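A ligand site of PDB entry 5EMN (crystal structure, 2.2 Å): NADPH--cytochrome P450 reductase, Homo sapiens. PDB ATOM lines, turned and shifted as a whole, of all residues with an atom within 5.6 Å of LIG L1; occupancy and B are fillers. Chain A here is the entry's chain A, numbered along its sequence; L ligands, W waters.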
ATOM      1  N   TYR A 119     -27.596  21.553  -8.920  1.00  0.00           N
ATOM      2  CA  TYR A 119     -29.028  21.835  -9.039  1.00  0.00           C
ATOM      3  C   TYR A 119     -29.593  21.034 -10.206  1.00  0.00           C
ATOM      4  O   TYR A 119     -28.852  20.624 -11.100  1.00  0.00           O
ATOM      5  CB  TYR A 119     -29.268  23.329  -9.262  1.00  0.00           C
ATOM      6  CG  TYR A 119     -29.056  24.161  -8.021  1.00  0.00           C
ATOM      7  CD1 TYR A 119     -30.051  24.252  -7.048  1.00  0.00           C
ATOM      8  CD2 TYR A 119     -27.843  24.816  -7.794  1.00  0.00           C
ATOM      9  CE1 TYR A 119     -29.836  24.976  -5.876  1.00  0.00           C
ATOM     10  CE2 TYR A 119     -27.631  25.530  -6.621  1.00  0.00           C
ATOM     11  CZ  TYR A 119     -28.620  25.608  -5.669  1.00  0.00           C
ATOM     12  OH  TYR A 119     -28.404  26.301  -4.501  1.00  0.00           O
ATOM     13  N   HIS A 260     -38.452  31.558   2.286  1.00  0.00           N
ATOM     14  CA  HIS A 260     -37.161  31.861   2.856  1.00  0.00           C
ATOM     15  C   HIS A 260     -37.190  33.255   3.467  1.00  0.00           C
ATOM     16  O   HIS A 260     -37.984  34.108   3.081  1.00  0.00           O
ATOM     17  CB  HIS A 260     -36.064  31.813   1.785  1.00  0.00           C
ATOM     18  CG  HIS A 260     -35.986  30.512   1.048  1.00  0.00           C
ATOM     19  ND1 HIS A 260     -35.872  29.291   1.684  1.00  0.00           N
ATOM     20  CD2 HIS A 260     -35.972  30.239  -0.285  1.00  0.00           C
ATOM     21  CE1 HIS A 260     -35.785  28.325   0.779  1.00  0.00           C
ATOM     22  NE2 HIS A 260     -35.841  28.878  -0.418  1.00  0.00           N
ATOM     23  N   THR A 319     -15.011  39.182   3.540  1.00  0.00           N
ATOM     24  CA  THR A 319     -14.684  37.817   3.969  1.00  0.00           C
ATOM     25  C   THR A 319     -14.497  36.815   2.850  1.00  0.00           C
ATOM     26  O   THR A 319     -13.677  35.893   2.924  1.00  0.00           O
ATOM     27  CB  THR A 319     -15.751  37.286   4.903  1.00  0.00           C
ATOM     28  OG1 THR A 319     -17.038  37.503   4.312  1.00  0.00           O
ATOM     29  CG2 THR A 319     -15.672  37.970   6.257  1.00  0.00           C
ATOM     30  N   ARG A 365      -8.668  29.967   1.308  1.00  0.00           N
ATOM     31  CA  ARG A 365      -9.778  30.796   1.762  1.00  0.00           C
ATOM     32  C   ARG A 365      -9.318  32.088   2.437  1.00  0.00           C
ATOM     33  O   ARG A 365      -9.792  32.441   3.503  1.00  0.00           O
ATOM     34  CB  ARG A 365     -10.638  29.996   2.748  1.00  0.00           C
ATOM     35  CG  ARG A 365     -11.323  28.790   2.148  1.00  0.00           C
ATOM     36  CD  ARG A 365     -12.596  29.182   1.459  1.00  0.00           C
ATOM     37  NE  ARG A 365     -13.452  28.030   1.245  1.00  0.00           N
ATOM     38  CZ  ARG A 365     -13.290  27.126   0.281  1.00  0.00           C
ATOM     39  NH1 ARG A 365     -14.124  26.110   0.186  1.00  0.00           N
ATOM     40  NH2 ARG A 365     -12.306  27.248  -0.602  1.00  0.00           N
ATOM     41  N   ARG A 395     -28.273  36.736   3.411  1.00  0.00           N
ATOM     42  CA  ARG A 395     -28.198  35.279   3.489  1.00  0.00           C
ATOM     43  C   ARG A 395     -29.617  34.748   3.649  1.00  0.00           C
ATOM     44  O   ARG A 395     -30.387  35.271   4.462  1.00  0.00           O
ATOM     45  CB  ARG A 395     -27.342  34.839   4.690  1.00  0.00           C
ATOM     46  CG  ARG A 395     -25.895  34.603   4.359  1.00  0.00           C
ATOM     47  CD  ARG A 395     -25.152  35.856   3.907  1.00  0.00           C
ATOM     48  NE  ARG A 395     -23.736  35.573   3.692  1.00  0.00           N
ATOM     49  CZ  ARG A 395     -22.833  36.466   3.282  1.00  0.00           C
ATOM     50  NH1 ARG A 395     -21.563  36.096   3.132  1.00  0.00           N
ATOM     51  NH2 ARG A 395     -23.188  37.715   3.024  1.00  0.00           N
ATOM     52  N   TYR A 396     -29.948  33.729   2.879  1.00  0.00           N
ATOM     53  CA  TYR A 396     -31.287  33.130   2.906  1.00  0.00           C
ATOM     54  C   TYR A 396     -31.347  31.972   3.891  1.00  0.00           C
ATOM     55  O   TYR A 396     -30.392  31.188   4.023  1.00  0.00           O
ATOM     56  CB  TYR A 396     -31.665  32.630   1.503  1.00  0.00           C
ATOM     57  CG  TYR A 396     -31.638  33.707   0.430  1.00  0.00           C
ATOM     58  CD1 TYR A 396     -32.650  34.681   0.358  1.00  0.00           C
ATOM     59  CD2 TYR A 396     -30.555  33.819  -0.449  1.00  0.00           C
ATOM     60  CE1 TYR A 396     -32.581  35.729  -0.568  1.00  0.00           C
ATOM     61  CE2 TYR A 396     -30.479  34.864  -1.382  1.00  0.00           C
ATOM     62  CZ  TYR A 396     -31.496  35.821  -1.424  1.00  0.00           C
ATOM     63  OH  TYR A 396     -31.380  36.905  -2.280  1.00  0.00           O
ATOM     64  N   TYR A 397     -32.479  31.846   4.570  1.00  0.00           N
ATOM     65  CA  TYR A 397     -32.691  30.779   5.513  1.00  0.00           C
ATOM     66  C   TYR A 397     -34.110  30.313   5.291  1.00  0.00           C
ATOM     67  O   TYR A 397     -34.978  31.104   4.949  1.00  0.00           O
ATOM     68  CB  TYR A 397     -32.496  31.280   6.944  1.00  0.00           C
ATOM     69  CG  TYR A 397     -31.057  31.611   7.199  1.00  0.00           C
ATOM     70  CD1 TYR A 397     -30.140  30.602   7.511  1.00  0.00           C
ATOM     71  CD2 TYR A 397     -30.574  32.922   7.064  1.00  0.00           C
ATOM     72  CE1 TYR A 397     -28.792  30.884   7.666  1.00  0.00           C
ATOM     73  CE2 TYR A 397     -29.233  33.205   7.212  1.00  0.00           C
ATOM     74  CZ  TYR A 397     -28.338  32.190   7.517  1.00  0.00           C
ATOM     75  OH  TYR A 397     -27.007  32.453   7.645  1.00  0.00           O
ATOM     76  N   SER A 398     -34.319  29.006   5.452  1.00  0.00           N
ATOM     77  CA  SER A 398     -35.619  28.394   5.268  1.00  0.00           C
ATOM     78  C   SER A 398     -36.412  28.564   6.527  1.00  0.00           C
ATOM     79  O   SER A 398     -36.068  27.988   7.561  1.00  0.00           O
ATOM     80  CB  SER A 398     -35.432  26.916   4.976  1.00  0.00           C
ATOM     81  OG  SER A 398     -34.320  26.756   4.106  1.00  0.00           O
ATOM     82  N   CYS A 413     -33.388  28.319  11.759  1.00  0.00           N
ATOM     83  CA  CYS A 413     -32.581  27.227  12.294  1.00  0.00           C
ATOM     84  C   CYS A 413     -31.277  27.277  11.508  1.00  0.00           C
ATOM     85  O   CYS A 413     -31.294  27.061  10.289  1.00  0.00           O
ATOM     86  CB  CYS A 413     -33.285  25.897  12.058  1.00  0.00           C
ATOM     87  SG  CYS A 413     -32.287  24.420  12.376  1.00  0.00           S
ATOM     88  N   ALA A 414     -30.159  27.542  12.159  1.00  0.00           N
ATOM     89  CA  ALA A 414     -28.907  27.637  11.424  1.00  0.00           C
ATOM     90  C   ALA A 414     -27.678  27.113  12.136  1.00  0.00           C
ATOM     91  O   ALA A 414     -27.600  27.111  13.368  1.00  0.00           O
ATOM     92  CB  ALA A 414     -28.663  29.074  11.020  1.00  0.00           C
ATOM     93  N   VAL A 415     -26.697  26.668  11.348  1.00  0.00           N
ATOM     94  CA  VAL A 415     -25.453  26.170  11.902  1.00  0.00           C
ATOM     95  C   VAL A 415     -24.430  27.278  11.708  1.00  0.00           C
ATOM     96  O   VAL A 415     -24.338  27.847  10.622  1.00  0.00           O
ATOM     97  CB  VAL A 415     -24.961  24.854  11.199  1.00  0.00           C
ATOM     98  CG1 VAL A 415     -24.585  25.120   9.745  1.00  0.00           C
ATOM     99  CG2 VAL A 415     -23.763  24.297  11.948  1.00  0.00           C
ATOM    100  N   VAL A 417     -20.970  29.010  11.027  1.00  0.00           N
ATOM    101  CA  VAL A 417     -19.864  28.596  10.185  1.00  0.00           C
ATOM    102  C   VAL A 417     -18.547  29.087  10.741  1.00  0.00           C
ATOM    103  O   VAL A 417     -18.310  30.281  10.797  1.00  0.00           O
ATOM    104  CB  VAL A 417     -20.023  29.144   8.756  1.00  0.00           C
ATOM    105  CG1 VAL A 417     -18.699  29.070   8.017  1.00  0.00           C
ATOM    106  CG2 VAL A 417     -21.084  28.349   8.030  1.00  0.00           C
ATOM    107  N   TYR A 419     -14.233  27.686  10.882  1.00  0.00           N
ATOM    108  CA  TYR A 419     -13.248  26.649  10.567  1.00  0.00           C
ATOM    109  C   TYR A 419     -11.841  27.221  10.518  1.00  0.00           C
ATOM    110  O   TYR A 419     -11.654  28.431  10.499  1.00  0.00           O
ATOM    111  CB  TYR A 419     -13.549  26.013   9.214  1.00  0.00           C
ATOM    112  CG  TYR A 419     -13.657  27.023   8.091  1.00  0.00           C
ATOM    113  CD1 TYR A 419     -14.827  27.767   7.903  1.00  0.00           C
ATOM    114  CD2 TYR A 419     -12.584  27.261   7.224  1.00  0.00           C
ATOM    115  CE1 TYR A 419     -14.929  28.733   6.891  1.00  0.00           C
ATOM    116  CE2 TYR A 419     -12.673  28.224   6.212  1.00  0.00           C
ATOM    117  CZ  TYR A 419     -13.852  28.962   6.045  1.00  0.00           C
ATOM    118  OH  TYR A 419     -13.934  29.937   5.083  1.00  0.00           O
ATOM    119  N   LYS A 428     -14.614  32.962  10.050  1.00  0.00           N
ATOM    120  CA  LYS A 428     -15.951  32.966  10.618  1.00  0.00           C
ATOM    121  C   LYS A 428     -17.006  33.368   9.589  1.00  0.00           C
ATOM    122  O   LYS A 428     -16.827  34.346   8.879  1.00  0.00           O
ATOM    123  CB  LYS A 428     -16.010  33.904  11.803  1.00  0.00           C
ATOM    124  CG  LYS A 428     -15.195  33.441  12.983  1.00  0.00           C
ATOM    125  CD  LYS A 428     -15.714  34.075  14.245  1.00  0.00           C
ATOM    126  CE  LYS A 428     -14.844  33.734  15.431  1.00  0.00           C
ATOM    127  NZ  LYS A 428     -15.357  34.425  16.653  1.00  0.00           N
ATOM    128  N   GLY A 429     -18.087  32.593   9.513  1.00  0.00           N
ATOM    129  CA  GLY A 429     -19.162  32.894   8.583  1.00  0.00           C
ATOM    130  C   GLY A 429     -19.825  34.205   8.968  1.00  0.00           C
ATOM    131  O   GLY A 429     -20.162  34.443  10.127  1.00  0.00           O
ATOM    132  N   VAL A 430     -20.030  35.072   7.980  1.00  0.00           N
ATOM    133  CA  VAL A 430     -20.605  36.385   8.248  1.00  0.00           C
ATOM    134  C   VAL A 430     -21.974  36.433   8.902  1.00  0.00           C
ATOM    135  O   VAL A 430     -22.111  36.982  10.003  1.00  0.00           O
ATOM    136  CB  VAL A 430     -20.645  37.225   6.950  1.00  0.00           C
ATOM    137  CG1 VAL A 430     -21.379  38.541   7.196  1.00  0.00           C
ATOM    138  CG2 VAL A 430     -19.227  37.499   6.491  1.00  0.00           C
ATOM    139  N   ALA A 431     -22.988  35.878   8.244  1.00  0.00           N
ATOM    140  CA  ALA A 431     -24.322  35.933   8.828  1.00  0.00           C
ATOM    141  C   ALA A 431     -24.525  35.060  10.069  1.00  0.00           C
ATOM    142  O   ALA A 431     -25.217  35.472  11.000  1.00  0.00           O
ATOM    143  CB  ALA A 431     -25.366  35.563   7.777  1.00  0.00           C
ATOM    144  N   THR A 432     -23.940  33.868  10.090  1.00  0.00           N
ATOM    145  CA  THR A 432     -24.149  33.010  11.244  1.00  0.00           C
ATOM    146  C   THR A 432     -23.482  33.510  12.524  1.00  0.00           C
ATOM    147  O   THR A 432     -24.077  33.429  13.592  1.00  0.00           O
ATOM    148  CB  THR A 432     -23.741  31.545  10.932  1.00  0.00           C
ATOM    149  OG1 THR A 432     -22.347  31.476  10.628  1.00  0.00           O
ATOM    150  CG2 THR A 432     -24.561  31.004   9.755  1.00  0.00           C
ATOM    151  N   ASN A 433     -22.275  34.053  12.447  1.00  0.00           N
ATOM    152  CA  ASN A 433     -21.682  34.566  13.688  1.00  0.00           C
ATOM    153  C   ASN A 433     -22.422  35.806  14.146  1.00  0.00           C
ATOM    154  O   ASN A 433     -22.537  36.080  15.340  1.00  0.00           O
ATOM    155  CB  ASN A 433     -20.188  34.863  13.500  1.00  0.00           C
ATOM    156  CG  ASN A 433     -19.329  33.640  13.785  1.00  0.00           C
ATOM    157  OD1 ASN A 433     -18.755  33.510  14.871  1.00  0.00           O
ATOM    158  ND2 ASN A 433     -19.263  32.726  12.824  1.00  0.00           N
ATOM    159  N   THR A 476     -29.457  20.912   9.094  1.00  0.00           N
ATOM    160  CA  THR A 476     -30.314  22.082   9.070  1.00  0.00           C
ATOM    161  C   THR A 476     -31.407  21.959   8.025  1.00  0.00           C
ATOM    162  O   THR A 476     -32.357  22.728   8.008  1.00  0.00           O
ATOM    163  CB  THR A 476     -29.529  23.380   8.815  1.00  0.00           C
ATOM    164  OG1 THR A 476     -28.704  23.220   7.649  1.00  0.00           O
ATOM    165  CG2 THR A 476     -28.670  23.711  10.039  1.00  0.00           C
ATOM    166  N   ALA A 479     -35.083  22.276   8.730  1.00  0.00           N
ATOM    167  CA  ALA A 479     -35.723  23.566   8.904  1.00  0.00           C
ATOM    168  C   ALA A 479     -37.159  23.792   8.406  1.00  0.00           C
ATOM    169  O   ALA A 479     -38.048  24.094   9.203  1.00  0.00           O
ATOM    170  CB  ALA A 479     -34.822  24.643   8.345  1.00  0.00           C
ATOM    171  N   ASP A 615     -35.179  22.015  -1.840  1.00  0.00           N
ATOM    172  CA  ASP A 615     -34.737  23.246  -1.210  1.00  0.00           C
ATOM    173  C   ASP A 615     -33.330  22.913  -0.725  1.00  0.00           C
ATOM    174  O   ASP A 615     -33.102  22.693   0.481  1.00  0.00           O
ATOM    175  CB  ASP A 615     -35.611  23.655  -0.023  1.00  0.00           C
ATOM    176  CG  ASP A 615     -35.124  24.941   0.654  1.00  0.00           C
ATOM    177  OD1 ASP A 615     -34.520  25.775  -0.048  1.00  0.00           O
ATOM    178  OD2 ASP A 615     -35.352  25.129   1.871  1.00  0.00           O
ATOM    179  N   VAL A 616     -32.397  22.848  -1.667  1.00  0.00           N
ATOM    180  CA  VAL A 616     -31.024  22.522  -1.327  1.00  0.00           C
ATOM    181  C   VAL A 616     -30.061  23.683  -1.528  1.00  0.00           C
ATOM    182  O   VAL A 616     -30.305  24.593  -2.315  1.00  0.00           O
ATOM    183  CB  VAL A 616     -30.529  21.290  -2.129  1.00  0.00           C
ATOM    184  CG1 VAL A 616     -31.349  20.070  -1.740  1.00  0.00           C
ATOM    185  CG2 VAL A 616     -30.639  21.547  -3.610  1.00  0.00           C
ATOM    186  N   TRP A 617     -28.951  23.626  -0.802  1.00  0.00           N
ATOM    187  CA  TRP A 617     -27.939  24.653  -0.862  1.00  0.00           C
ATOM    188  C   TRP A 617     -26.575  24.112  -0.406  1.00  0.00           C
ATOM    189  O   TRP A 617     -26.457  22.972   0.089  1.00  0.00           O
ATOM    190  CB  TRP A 617     -28.351  25.822   0.034  1.00  0.00           C
ATOM    191  CG  TRP A 617     -28.327  25.501   1.502  1.00  0.00           C
ATOM    192  CD1 TRP A 617     -27.210  25.459   2.306  1.00  0.00           C
ATOM    193  CD2 TRP A 617     -29.429  25.112   2.324  1.00  0.00           C
ATOM    194  NE1 TRP A 617     -27.567  25.063   3.580  1.00  0.00           N
ATOM    195  CE2 TRP A 617     -28.914  24.836   3.618  1.00  0.00           C
ATOM    196  CE3 TRP A 617     -30.808  24.965   2.093  1.00  0.00           C
ATOM    197  CZ2 TRP A 617     -29.725  24.421   4.675  1.00  0.00           C
ATOM    198  CZ3 TRP A 617     -31.617  24.560   3.149  1.00  0.00           C
ATOM    199  CH2 TRP A 617     -31.072  24.286   4.430  1.00  0.00           C
ATOM    200  N   SER A 618     -25.537  24.918  -0.597  1.00  0.00           N
ATOM    201  CA  SER A 618     -24.204  24.524  -0.188  1.00  0.00           C
ATOM    202  C   SER A 618     -23.392  25.795  -0.029  1.00  0.00           C
ATOM    203  O   SER A 618     -23.922  26.867  -0.422  1.00  0.00           O
ATOM    204  CB  SER A 618     -23.573  23.625  -1.232  1.00  0.00           C
ATOM    205  OG  SER A 618     -23.339  24.351  -2.424  1.00  0.00           O
ATOM    206  OXT SER A 618     -22.247  25.705   0.489  1.00  0.00           O
HETATM  207  P1  LIG L   1     -20.188  32.945   4.858  1.00  0.00           P
HETATM  208  O1  LIG L   1     -19.337  34.029   5.403  1.00  0.00           O
HETATM  209  O2  LIG L   1     -21.084  33.243   3.716  1.00  0.00           O
HETATM  210  O3  LIG L   1     -19.241  31.704   4.458  1.00  0.00           O
HETATM  211  C1  LIG L   1     -19.764  30.606   3.715  1.00  0.00           C
HETATM  212  C2  LIG L   1     -18.602  29.911   2.990  1.00  0.00           C
HETATM  213  O4  LIG L   1     -17.616  29.466   3.927  1.00  0.00           O
HETATM  214  C3  LIG L   1     -19.052  28.610   2.358  1.00  0.00           C
HETATM  215  O5  LIG L   1     -19.754  28.912   1.139  1.00  0.00           O
HETATM  216  C4  LIG L   1     -17.679  28.062   2.028  1.00  0.00           C
HETATM  217  O6  LIG L   1     -17.157  28.716   0.854  1.00  0.00           O
HETATM  218  C5  LIG L   1     -16.866  28.444   3.246  1.00  0.00           C
HETATM  219  N1  LIG L   1     -16.714  27.319   4.195  1.00  0.00           N
HETATM  220  C6  LIG L   1     -17.689  26.907   5.223  1.00  0.00           C
HETATM  221  N2  LIG L   1     -16.966  25.789   5.856  1.00  0.00           N
HETATM  222  C7  LIG L   1     -15.797  25.635   5.243  1.00  0.00           C
HETATM  223  C8  LIG L   1     -14.819  24.752   5.491  1.00  0.00           C
HETATM  224  N3  LIG L   1     -14.981  23.991   6.561  1.00  0.00           N
HETATM  225  N4  LIG L   1     -13.710  24.683   4.742  1.00  0.00           N
HETATM  226  C9  LIG L   1     -13.551  25.567   3.676  1.00  0.00           C
HETATM  227  N5  LIG L   1     -14.589  26.474   3.431  1.00  0.00           N
HETATM  228  C10 LIG L   1     -15.678  26.480   4.222  1.00  0.00           C
HETATM  229  N6  LIG L   1     -28.211  27.668   6.211  1.00  0.00           N
HETATM  230  C11 LIG L   1     -28.721  27.294   7.462  1.00  0.00           C
HETATM  231  O7  LIG L   1     -27.945  27.047   8.381  1.00  0.00           O
HETATM  232  N7  LIG L   1     -30.105  27.136   7.635  1.00  0.00           N
HETATM  233  C12 LIG L   1     -30.974  27.340   6.552  1.00  0.00           C
HETATM  234  O8  LIG L   1     -32.180  27.235   6.722  1.00  0.00           O
HETATM  235  C13 LIG L   1     -30.457  27.682   5.304  1.00  0.00           C
HETATM  236  N8  LIG L   1     -31.261  27.720   4.237  1.00  0.00           N
HETATM  237  C14 LIG L   1     -30.760  28.070   3.045  1.00  0.00           C
HETATM  238  C15 LIG L   1     -31.610  28.156   1.944  1.00  0.00           C
HETATM  239  C16 LIG L   1     -31.121  28.577   0.716  1.00  0.00           C
HETATM  240  C17 LIG L   1     -31.998  28.785  -0.346  1.00  0.00           C
HETATM  241  C18 LIG L   1     -29.771  28.889   0.578  1.00  0.00           C
HETATM  242  C19 LIG L   1     -29.261  29.306  -0.655  1.00  0.00           C
HETATM  243  C20 LIG L   1     -28.921  28.803   1.680  1.00  0.00           C
HETATM  244  C21 LIG L   1     -29.421  28.405   2.919  1.00  0.00           C
HETATM  245  N9  LIG L   1     -28.624  28.370   3.992  1.00  0.00           N
HETATM  246  C22 LIG L   1     -29.094  27.846   5.136  1.00  0.00           C
HETATM  247  C23 LIG L   1     -27.191  28.750   3.923  1.00  0.00           C
HETATM  248  C24 LIG L   1     -27.041  30.214   4.330  1.00  0.00           C
HETATM  249  O9  LIG L   1     -27.675  31.041   3.356  1.00  0.00           O
HETATM  250  C25 LIG L   1     -25.581  30.644   4.472  1.00  0.00           C
HETATM  251  O10 LIG L   1     -24.843  30.278   3.304  1.00  0.00           O
HETATM  252  C26 LIG L   1     -24.928  30.016   5.708  1.00  0.00           C
HETATM  253  O11 LIG L   1     -25.687  30.315   6.872  1.00  0.00           O
HETATM  254  C27 LIG L   1     -23.508  30.569   5.859  1.00  0.00           C
HETATM  255  O12 LIG L   1     -23.540  31.998   5.806  1.00  0.00           O
HETATM  256  P2  LIG L   1     -22.451  32.903   6.575  1.00  0.00           P
HETATM  257  O13 LIG L   1     -22.544  32.637   8.034  1.00  0.00           O
HETATM  258  O14 LIG L   1     -22.596  34.297   6.108  1.00  0.00           O
HETATM  259  O15 LIG L   1     -21.058  32.296   6.058  1.00  0.00           O
HETATM  260  N1  LG2 L   2     -27.842  27.263 -10.583  1.00  0.00           N
HETATM  261  C1  LG2 L   2     -28.299  26.501 -11.599  1.00  0.00           C
HETATM  262  O1  LG2 L   2     -27.564  26.151 -12.534  1.00  0.00           O
HETATM  263  N2  LG2 L   2     -29.623  26.117 -11.532  1.00  0.00           N
HETATM  264  C2  LG2 L   2     -30.550  26.430 -10.539  1.00  0.00           C
HETATM  265  O2  LG2 L   2     -31.659  25.972 -10.713  1.00  0.00           O
HETATM  266  C3  LG2 L   2     -30.085  27.216  -9.461  1.00  0.00           C
HETATM  267  N3  LG2 L   2     -31.002  27.522  -8.410  1.00  0.00           N
HETATM  268  C4  LG2 L   2     -30.444  28.283  -7.389  1.00  0.00           C
HETATM  269  C5  LG2 L   2     -31.330  28.616  -6.297  1.00  0.00           C
HETATM  270  C6  LG2 L   2     -30.884  29.387  -5.190  1.00  0.00           C
HETATM  271  C7  LG2 L   2     -31.918  29.671  -4.078  1.00  0.00           C
HETATM  272  C8  LG2 L   2     -29.477  29.886  -5.127  1.00  0.00           C
HETATM  273  C9  LG2 L   2     -28.915  30.636  -4.113  1.00  0.00           C
HETATM  274  C10 LG2 L   2     -28.627  29.575  -6.173  1.00  0.00           C
HETATM  275  C11 LG2 L   2     -29.059  28.787  -7.321  1.00  0.00           C
HETATM  276  N4  LG2 L   2     -28.199  28.427  -8.448  1.00  0.00           N
HETATM  277  C12 LG2 L   2     -28.707  27.608  -9.547  1.00  0.00           C
HETATM  278  C13 LG2 L   2     -26.823  28.895  -8.470  1.00  0.00           C
HETATM  279  C14 LG2 L   2     -26.696  30.343  -9.064  1.00  0.00           C
HETATM  280  O3  LG2 L   2     -27.236  30.342 -10.450  1.00  0.00           O
HETATM  281  C15 LG2 L   2     -25.244  30.767  -9.050  1.00  0.00           C
HETATM  282  O4  LG2 L   2     -24.845  30.759  -7.648  1.00  0.00           O
HETATM  283  C16 LG2 L   2     -25.117  32.202  -9.686  1.00  0.00           C
HETATM  284  O5  LG2 L   2     -23.677  32.415  -9.634  1.00  0.00           O
HETATM  285  C17 LG2 L   2     -25.693  33.330  -8.864  1.00  0.00           C
HETATM  286  O6  LG2 L   2     -25.563  34.627  -9.559  1.00  0.00           O
HETATM  287  P1  LG2 L   2     -26.009  36.027  -8.981  1.00  0.00           P
HETATM  288  O7  LG2 L   2     -25.116  36.385  -7.850  1.00  0.00           O
HETATM  289  O8  LG2 L   2     -27.548  35.877  -8.736  1.00  0.00           O
HETATM  290  O9  LG2 L   2     -25.645  36.978 -10.221  1.00  0.00           O
HETATM  291  O   HOH W   1     -33.777  28.476   9.025  1.00  0.00           O
HETATM  292  O   HOH W   2     -15.936  31.647   4.824  1.00  0.00           O
HETATM  293  O   HOH W   3     -25.516  27.875   8.141  1.00  0.00           O
HETATM  294  O   HOH W   4     -17.871  35.208   3.390  1.00  0.00           O
HETATM  295  O   HOH W   5     -16.296  23.977   1.756  1.00  0.00           O
HETATM  296  O   HOH W   6     -23.230  32.222   2.407  1.00  0.00           O
HETATM  297  O   HOH W   7     -27.648  32.505   1.230  1.00  0.00           O
HETATM  298  O   HOH W   8     -14.967  30.387   0.472  1.00  0.00           O
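O11 of LIG L1 is in hydrogen-bond range of OH of Tyr 397 (2.6 Å). N of Ala 431 sits at hydrogen-bond distance from O14 of LIG L1 (2.7 Å). The backbone NH (N) of Thr 432 lies within hydrogen-bond range of an oxygen (O13) of LIG L1 (2.8 Å). The side-chain hydroxyl (OG1) of Thr 432 lies within hydrogen-bond range of an oxygen (O13) of LIG L1, at 2.8 Å. O of Tyr 396 is in hydrogen-bond range of O9 of LIG L1 (2.8 Å). An oxygen (O1) of LIG L1 lies within hydrogen-bond range of the backbone NH (N) of Val 430. The backbone carbonyl oxygen of Cys 413 sits at hydrogen-bond distance from a nitrogen (N7) of LIG L1 (2.9 Å). The guanidinium group of Arg 365 is in hydrogen-bond range of a nitrogen (N5) of LIG L1 (2.9 Å). An oxygen (O2) of LIG L1 is in salt-bridge range of the guanidinium group of Arg 395 (3.0 Å). N of Ser 398 lies within hydrogen-bond range of O8 of LIG L1. N8 of LIG L1 lies within hydrogen-bond range of OG of Ser 398. N of Val 415 sits at hydrogen-bond distance from O7 of LIG L1 (3.2 Å).
OG1 of Thr 432 is in hydrogen-bond range of N of Val 417 (2.9 Å). The side-chain carboxylate (OD2) of Asp 615 sits at hydrogen-bond distance from the side-chain hydroxyl (OG) of Ser 398. The backbone carbonyl oxygen (O) of Val 417 is in hydrogen-bond range of the backbone NH (N) of Gly 429 (2.7 Å). The backbone carbonyl oxygen (O) of Gly 429 is in hydrogen-bond range of the side-chain amide nitrogen (ND2) of Asn 433, at 3.3 Å. O of Val 417 lies within hydrogen-bond range of ND2 of Asn 433 (3.3 Å). A ring nitrogen (NE2) of His 260 lies close to the side-chain carboxylate (OD1) of Asp 615 (3.4 Å).
A nitrogen (N9) of LIG L1 lies close to the indole nitrogen of Trp 617 (3.5 Å). Merely in contact with LIG L1: His 260 (3.8 Å), Ala 414 (3.2 Å), Val 417 (3.7 Å), Tyr 419 (3.5 Å), Gly 429 (3.2 Å), Thr 476 (3.8 Å) and Asp 615 (3.9 Å). Of the 25 residues printed, 18 come within 4 Å of LIG L1. The nearest printed residue that does not touch LIG L1 is Ala 479 (4.04 Å).
Water W3 lies within hydrogen-bond range of an oxygen (O7) of LIG L1 and the backbone carbonyl oxygen (O) of Val 415. Water W7 bridges an oxygen (O9) of LIG L1 (2.6 Å) and the backbone NH (N) of Tyr 396 (3.1 Å). Water W4 lies within hydrogen-bond range of the side-chain hydroxyl (OG1) of Thr 319 (2.6 Å) and an oxygen (O1) of LIG L1 (2.8 Å). Water W8 bridges O6 of LIG L1 (2.8 Å) and NE of Arg 365 (2.9 Å). Water W1 lies within hydrogen-bond range of the backbone carbonyl oxygen (O) of Ser 398 (2.8 Å), the backbone NH (N) of Cys 413 (2.8 Å) and an oxygen (O8) of LIG L1 (3.1 Å). Water W5 lies within hydrogen-bond range of the guanidinium group (NH1) of Arg 365 (3.4 Å) and a nitrogen (N5) of LIG L1 (3.5 Å).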
